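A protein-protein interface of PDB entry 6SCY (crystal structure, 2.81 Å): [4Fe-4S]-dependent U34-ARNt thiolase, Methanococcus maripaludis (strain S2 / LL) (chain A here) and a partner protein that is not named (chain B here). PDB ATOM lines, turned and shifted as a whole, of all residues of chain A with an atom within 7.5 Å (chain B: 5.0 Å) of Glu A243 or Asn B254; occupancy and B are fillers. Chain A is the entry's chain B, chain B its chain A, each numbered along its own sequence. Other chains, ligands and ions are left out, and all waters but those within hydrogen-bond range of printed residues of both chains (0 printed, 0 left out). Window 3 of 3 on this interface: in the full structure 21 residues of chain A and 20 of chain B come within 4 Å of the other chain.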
ATOM      1  N   GLN A 176     -10.775 -18.965 -17.515  1.00  0.00           N
ATOM      2  CA  GLN A 176      -9.741 -19.957 -17.240  1.00  0.00           C
ATOM      3  C   GLN A 176      -9.676 -20.228 -15.759  1.00  0.00           C
ATOM      4  O   GLN A 176      -9.746 -21.377 -15.361  1.00  0.00           O
ATOM      5  CB  GLN A 176      -8.366 -19.469 -17.714  1.00  0.00           C
ATOM      6  CG  GLN A 176      -7.968 -19.979 -19.079  1.00  0.00           C
ATOM      7  CD  GLN A 176      -7.616 -18.850 -20.008  1.00  0.00           C
ATOM      8  OE1 GLN A 176      -6.690 -18.073 -19.760  1.00  0.00           O
ATOM      9  NE2 GLN A 176      -8.352 -18.730 -21.098  1.00  0.00           N
ATOM     10  N   ILE A 183     -12.212 -27.617 -12.078  1.00  0.00           N
ATOM     11  CA  ILE A 183     -11.444 -28.855 -12.327  1.00  0.00           C
ATOM     12  C   ILE A 183     -10.668 -29.301 -11.070  1.00  0.00           C
ATOM     13  O   ILE A 183     -10.596 -30.497 -10.797  1.00  0.00           O
ATOM     14  CB  ILE A 183     -10.537 -28.762 -13.599  1.00  0.00           C
ATOM     15  CG1 ILE A 183     -11.369 -28.460 -14.868  1.00  0.00           C
ATOM     16  CG2 ILE A 183      -9.704 -30.044 -13.797  1.00  0.00           C
ATOM     17  CD1 ILE A 183     -10.633 -27.756 -15.971  1.00  0.00           C
ATOM     18  N   LEU A 238       3.193 -22.615 -15.826  1.00  0.00           N
ATOM     19  CA  LEU A 238       2.152 -23.558 -15.462  1.00  0.00           C
ATOM     20  C   LEU A 238       1.432 -23.968 -16.759  1.00  0.00           C
ATOM     21  O   LEU A 238       0.794 -23.142 -17.418  1.00  0.00           O
ATOM     22  CB  LEU A 238       1.217 -22.969 -14.387  1.00  0.00           C
ATOM     23  CG  LEU A 238       0.330 -23.968 -13.602  1.00  0.00           C
ATOM     24  CD1 LEU A 238       0.524 -23.857 -12.040  1.00  0.00           C
ATOM     25  CD2 LEU A 238      -1.128 -23.767 -14.048  1.00  0.00           C
ATOM     26  N   SER A 239       1.581 -25.248 -17.131  1.00  0.00           N
ATOM     27  CA  SER A 239       0.988 -25.838 -18.324  1.00  0.00           C
ATOM     28  C   SER A 239      -0.515 -26.116 -18.184  1.00  0.00           C
ATOM     29  O   SER A 239      -1.174 -26.309 -19.202  1.00  0.00           O
ATOM     30  CB  SER A 239       1.736 -27.107 -18.716  1.00  0.00           C
ATOM     31  OG  SER A 239       3.113 -26.852 -18.938  1.00  0.00           O
ATOM     32  N   PHE A 240      -1.058 -26.137 -16.946  1.00  0.00           N
ATOM     33  CA  PHE A 240      -2.484 -26.379 -16.691  1.00  0.00           C
ATOM     34  C   PHE A 240      -3.376 -25.257 -17.237  1.00  0.00           C
ATOM     35  O   PHE A 240      -4.389 -25.556 -17.870  1.00  0.00           O
ATOM     36  CB  PHE A 240      -2.751 -26.658 -15.195  1.00  0.00           C
ATOM     37  CG  PHE A 240      -4.171 -27.026 -14.821  1.00  0.00           C
ATOM     38  CD1 PHE A 240      -4.877 -27.977 -15.551  1.00  0.00           C
ATOM     39  CD2 PHE A 240      -4.783 -26.463 -13.705  1.00  0.00           C
ATOM     40  CE1 PHE A 240      -6.177 -28.331 -15.193  1.00  0.00           C
ATOM     41  CE2 PHE A 240      -6.082 -26.819 -13.344  1.00  0.00           C
ATOM     42  CZ  PHE A 240      -6.770 -27.748 -14.091  1.00  0.00           C
ATOM     43  N   ARG A 241      -2.982 -23.978 -17.021  1.00  0.00           N
ATOM     44  CA  ARG A 241      -3.704 -22.804 -17.518  1.00  0.00           C
ATOM     45  C   ARG A 241      -3.714 -22.794 -19.052  1.00  0.00           C
ATOM     46  O   ARG A 241      -4.749 -22.485 -19.643  1.00  0.00           O
ATOM     47  CB  ARG A 241      -3.137 -21.490 -16.945  1.00  0.00           C
ATOM     48  CG  ARG A 241      -4.118 -20.319 -17.026  1.00  0.00           C
ATOM     49  CD  ARG A 241      -3.594 -19.062 -16.362  1.00  0.00           C
ATOM     50  NE  ARG A 241      -4.618 -18.018 -16.248  1.00  0.00           N
ATOM     51  CZ  ARG A 241      -5.159 -17.612 -15.100  1.00  0.00           C
ATOM     52  NH1 ARG A 241      -6.081 -16.659 -15.095  1.00  0.00           N
ATOM     53  NH2 ARG A 241      -4.778 -18.151 -13.947  1.00  0.00           N
ATOM     54  N   SER A 242      -2.588 -23.183 -19.693  1.00  0.00           N
ATOM     55  CA  SER A 242      -2.489 -23.275 -21.154  1.00  0.00           C
ATOM     56  C   SER A 242      -3.338 -24.444 -21.696  1.00  0.00           C
ATOM     57  O   SER A 242      -3.764 -24.399 -22.852  1.00  0.00           O
ATOM     58  CB  SER A 242      -1.036 -23.381 -21.605  1.00  0.00           C
ATOM     59  OG  SER A 242      -0.421 -24.567 -21.132  1.00  0.00           O
ATOM     60  N   GLU A 243      -3.609 -25.468 -20.848  1.00  0.00           N
ATOM     61  CA  GLU A 243      -4.449 -26.616 -21.197  1.00  0.00           C
ATOM     62  C   GLU A 243      -5.917 -26.197 -21.058  1.00  0.00           C
ATOM     63  O   GLU A 243      -6.720 -26.483 -21.952  1.00  0.00           O
ATOM     64  CB  GLU A 243      -4.131 -27.825 -20.299  1.00  0.00           C
ATOM     65  CG  GLU A 243      -4.641 -29.147 -20.853  1.00  0.00           C
ATOM     66  CD  GLU A 243      -4.687 -30.313 -19.881  1.00  0.00           C
ATOM     67  OE1 GLU A 243      -3.653 -30.611 -19.241  1.00  0.00           O
ATOM     68  OE2 GLU A 243      -5.762 -30.950 -19.782  1.00  0.00           O
ATOM     69  N   VAL A 244      -6.252 -25.504 -19.939  1.00  0.00           N
ATOM     70  CA  VAL A 244      -7.589 -24.981 -19.614  1.00  0.00           C
ATOM     71  C   VAL A 244      -8.026 -23.941 -20.648  1.00  0.00           C
ATOM     72  O   VAL A 244      -9.183 -23.961 -21.064  1.00  0.00           O
ATOM     73  CB  VAL A 244      -7.674 -24.464 -18.148  1.00  0.00           C
ATOM     74  CG1 VAL A 244      -8.896 -23.582 -17.914  1.00  0.00           C
ATOM     75  CG2 VAL A 244      -7.662 -25.625 -17.161  1.00  0.00           C
ATOM     76  N   SER A 245      -7.091 -23.061 -21.087  1.00  0.00           N
ATOM     77  CA  SER A 245      -7.354 -22.030 -22.102  1.00  0.00           C
ATOM     78  C   SER A 245      -7.791 -22.671 -23.406  1.00  0.00           C
ATOM     79  O   SER A 245      -8.725 -22.183 -24.031  1.00  0.00           O
ATOM     80  CB  SER A 245      -6.134 -21.144 -22.324  1.00  0.00           C
ATOM     81  OG  SER A 245      -5.062 -21.862 -22.911  1.00  0.00           O
ATOM     82  N   ASP A 246      -7.165 -23.806 -23.766  1.00  0.00           N
ATOM     83  CA  ASP A 246      -7.485 -24.588 -24.957  1.00  0.00           C
ATOM     84  C   ASP A 246      -8.877 -25.200 -24.841  1.00  0.00           C
ATOM     85  O   ASP A 246      -9.588 -25.274 -25.843  1.00  0.00           O
ATOM     86  CB  ASP A 246      -6.411 -25.663 -25.207  1.00  0.00           C
ATOM     87  CG  ASP A 246      -5.227 -25.194 -26.050  1.00  0.00           C
ATOM     88  OD1 ASP A 246      -4.912 -25.866 -27.059  1.00  0.00           O
ATOM     89  OD2 ASP A 246      -4.614 -24.151 -25.700  1.00  0.00           O
ATOM     90  N   ILE A 247      -9.280 -25.587 -23.613  1.00  0.00           N
ATOM     91  CA  ILE A 247     -10.606 -26.143 -23.325  1.00  0.00           C
ATOM     92  C   ILE A 247     -11.673 -25.060 -23.565  1.00  0.00           C
ATOM     93  O   ILE A 247     -12.605 -25.288 -24.341  1.00  0.00           O
ATOM     94  CB  ILE A 247     -10.667 -26.769 -21.892  1.00  0.00           C
ATOM     95  CG1 ILE A 247      -9.755 -28.026 -21.779  1.00  0.00           C
ATOM     96  CG2 ILE A 247     -12.113 -27.077 -21.466  1.00  0.00           C
ATOM     97  CD1 ILE A 247      -9.255 -28.357 -20.381  1.00  0.00           C
ATOM     98  N   THR A 248     -11.510 -23.880 -22.927  1.00  0.00           N
ATOM     99  CA  THR A 248     -12.421 -22.730 -23.053  1.00  0.00           C
ATOM    100  C   THR A 248     -12.470 -22.220 -24.490  1.00  0.00           C
ATOM    101  O   THR A 248     -13.550 -21.852 -24.961  1.00  0.00           O
ATOM    102  CB  THR A 248     -12.051 -21.589 -22.081  1.00  0.00           C
ATOM    103  OG1 THR A 248     -10.748 -21.094 -22.387  1.00  0.00           O
ATOM    104  CG2 THR A 248     -12.133 -21.992 -20.612  1.00  0.00           C
ATOM    105  N   ASP A 249     -11.298 -22.199 -25.183  1.00  0.00           N
ATOM    106  CA  ASP A 249     -11.202 -21.759 -26.578  1.00  0.00           C
ATOM    107  C   ASP A 249     -11.990 -22.696 -27.484  1.00  0.00           C
ATOM    108  O   ASP A 249     -12.826 -22.208 -28.243  1.00  0.00           O
ATOM    109  CB  ASP A 249      -9.742 -21.633 -27.060  1.00  0.00           C
ATOM    110  CG  ASP A 249      -8.991 -20.402 -26.566  1.00  0.00           C
ATOM    111  OD1 ASP A 249      -9.628 -19.333 -26.410  1.00  0.00           O
ATOM    112  OD2 ASP A 249      -7.762 -20.506 -26.342  1.00  0.00           O
ATOM    113  N   ASN B 250      -9.680 -36.142 -21.647  1.00  0.00           N
ATOM    114  CA  ASN B 250      -8.375 -35.514 -21.902  1.00  0.00           C
ATOM    115  C   ASN B 250      -7.793 -34.847 -20.658  1.00  0.00           C
ATOM    116  O   ASN B 250      -6.573 -34.724 -20.555  1.00  0.00           O
ATOM    117  CB  ASN B 250      -8.414 -34.566 -23.093  1.00  0.00           C
ATOM    118  CG  ASN B 250      -8.016 -35.245 -24.381  1.00  0.00           C
ATOM    119  OD1 ASN B 250      -8.846 -35.816 -25.089  1.00  0.00           O
ATOM    120  ND2 ASN B 250      -6.726 -35.223 -24.701  1.00  0.00           N
ATOM    121  N   LEU B 251      -8.656 -34.469 -19.699  1.00  0.00           N
ATOM    122  CA  LEU B 251      -8.231 -33.898 -18.428  1.00  0.00           C
ATOM    123  C   LEU B 251      -7.671 -35.011 -17.551  1.00  0.00           C
ATOM    124  O   LEU B 251      -6.656 -34.805 -16.897  1.00  0.00           O
ATOM    125  CB  LEU B 251      -9.390 -33.191 -17.711  1.00  0.00           C
ATOM    126  CG  LEU B 251      -9.570 -31.719 -18.002  1.00  0.00           C
ATOM    127  CD1 LEU B 251     -10.919 -31.272 -17.559  1.00  0.00           C
ATOM    128  CD2 LEU B 251      -8.522 -30.886 -17.297  1.00  0.00           C
ATOM    129  N   GLU B 252      -8.333 -36.186 -17.555  1.00  0.00           N
ATOM    130  CA  GLU B 252      -7.940 -37.386 -16.802  1.00  0.00           C
ATOM    131  C   GLU B 252      -6.624 -37.957 -17.381  1.00  0.00           C
ATOM    132  O   GLU B 252      -5.704 -38.311 -16.628  1.00  0.00           O
ATOM    133  CB  GLU B 252      -9.082 -38.428 -16.850  1.00  0.00           C
ATOM    134  CG  GLU B 252      -8.891 -39.665 -15.989  1.00  0.00           C
ATOM    135  CD  GLU B 252      -8.825 -39.464 -14.489  1.00  0.00           C
ATOM    136  OE1 GLU B 252      -9.678 -38.735 -13.933  1.00  0.00           O
ATOM    137  OE2 GLU B 252      -7.923 -40.063 -13.862  1.00  0.00           O
ATOM    138  N   LYS B 253      -6.536 -37.984 -18.726  1.00  0.00           N
ATOM    139  CA  LYS B 253      -5.392 -38.453 -19.507  1.00  0.00           C
ATOM    140  C   LYS B 253      -4.121 -37.612 -19.269  1.00  0.00           C
ATOM    141  O   LYS B 253      -3.025 -38.108 -19.525  1.00  0.00           O
ATOM    142  CB  LYS B 253      -5.744 -38.486 -21.012  1.00  0.00           C
ATOM    143  CG  LYS B 253      -6.515 -39.714 -21.490  1.00  0.00           C
ATOM    144  CD  LYS B 253      -5.603 -40.855 -21.964  1.00  0.00           C
ATOM    145  CE  LYS B 253      -5.458 -41.930 -20.914  1.00  0.00           C
ATOM    146  NZ  LYS B 253      -4.511 -42.991 -21.343  1.00  0.00           N
ATOM    147  N   ASN B 254      -4.259 -36.361 -18.782  1.00  0.00           N
ATOM    148  CA  ASN B 254      -3.126 -35.461 -18.495  1.00  0.00           C
ATOM    149  C   ASN B 254      -2.922 -35.221 -17.003  1.00  0.00           C
ATOM    150  O   ASN B 254      -1.802 -34.953 -16.569  1.00  0.00           O
ATOM    151  CB  ASN B 254      -3.282 -34.126 -19.223  1.00  0.00           C
ATOM    152  CG  ASN B 254      -2.855 -34.157 -20.671  1.00  0.00           C
ATOM    153  OD1 ASN B 254      -1.783 -34.665 -21.027  1.00  0.00           O
ATOM    154  ND2 ASN B 254      -3.679 -33.595 -21.539  1.00  0.00           N
ATOM    155  N   HIS B 255      -4.015 -35.288 -16.230  1.00  0.00           N
ATOM    156  CA  HIS B 255      -4.036 -35.080 -14.783  1.00  0.00           C
ATOM    157  C   HIS B 255      -4.882 -36.196 -14.160  1.00  0.00           C
ATOM    158  O   HIS B 255      -6.109 -36.084 -14.120  1.00  0.00           O
ATOM    159  CB  HIS B 255      -4.608 -33.696 -14.428  1.00  0.00           C
ATOM    160  CG  HIS B 255      -3.915 -32.559 -15.114  1.00  0.00           C
ATOM    161  ND1 HIS B 255      -2.965 -31.799 -14.462  1.00  0.00           N
ATOM    162  CD2 HIS B 255      -4.060 -32.089 -16.376  1.00  0.00           C
ATOM    163  CE1 HIS B 255      -2.566 -30.892 -15.340  1.00  0.00           C
ATOM    164  NE2 HIS B 255      -3.188 -31.034 -16.510  1.00  0.00           N
ATOM    165  N   PRO B 256      -4.244 -37.300 -13.714  1.00  0.00           N
ATOM    166  CA  PRO B 256      -5.007 -38.416 -13.134  1.00  0.00           C
ATOM    167  C   PRO B 256      -5.757 -38.070 -11.848  1.00  0.00           C
ATOM    168  O   PRO B 256      -5.168 -37.569 -10.890  1.00  0.00           O
ATOM    169  CB  PRO B 256      -3.935 -39.488 -12.897  1.00  0.00           C
ATOM    170  CG  PRO B 256      -2.769 -39.085 -13.732  1.00  0.00           C
ATOM    171  CD  PRO B 256      -2.798 -37.595 -13.715  1.00  0.00           C
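NE2 of His B255 sits at hydrogen-bond distance from OE1 of Glu A243, at 2.8 Å.
The backbone carbonyl oxygen of Asn B250 lies within hydrogen-bond range of the side-chain amide nitrogen of Asn B254 (3.3 Å).
CD2 of Leu B251 touches CG2 of Ile A183 (3.8 Å).
CD1 of Phe A240 touches NE2 of His B255, 3.6 Å away.
Asn B250 touches Glu A243.
CD2 of Leu B251 touches OE2 of Glu A243 (3.7 Å).
Glu A243 touches Asn B254 (OE1 to CB, 3.5 Å).
Of the printed residues of chain B, Glu A243 touches Asn B250, Leu B251, Asn B254 and His B255.
Of chain A, only Glu A243 comes within 4 Å of Asn B254.
Of the printed residues of chain A, Asn B250 touches Glu A243.
Of the printed residues of chain B, Ile A183 touches Leu B251 (3.8 Å).
Printed residues of chain B within 4 Å of Phe A240: His B255 (3.6 Å).
Of the printed residues of chain A, Leu B251 touches Ile A183 (3.8 Å) and Glu A243 (3.7 Å).
The nearest printed residue of chain B that does not touch Phe A240 is Leu B251 (4.1 Å).
Hydrophobic or aromatic side chains of chain A that line the printed part of chain B: Ile A183 and Phe A240.
Of the 7 printed residues of chain B, 4 touch a printed residue of chain A.
Hydrophobic or aromatic side chains of chain B within 4 Å of the printed part of chain A: Leu B251 and His B255.
Among the printed residues, 6 pairs touch across the chains.
Among the printed residues, no Asp or Glu carboxylate lies within 4 Å of a Lys or Arg side-chain nitrogen of the other chain.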
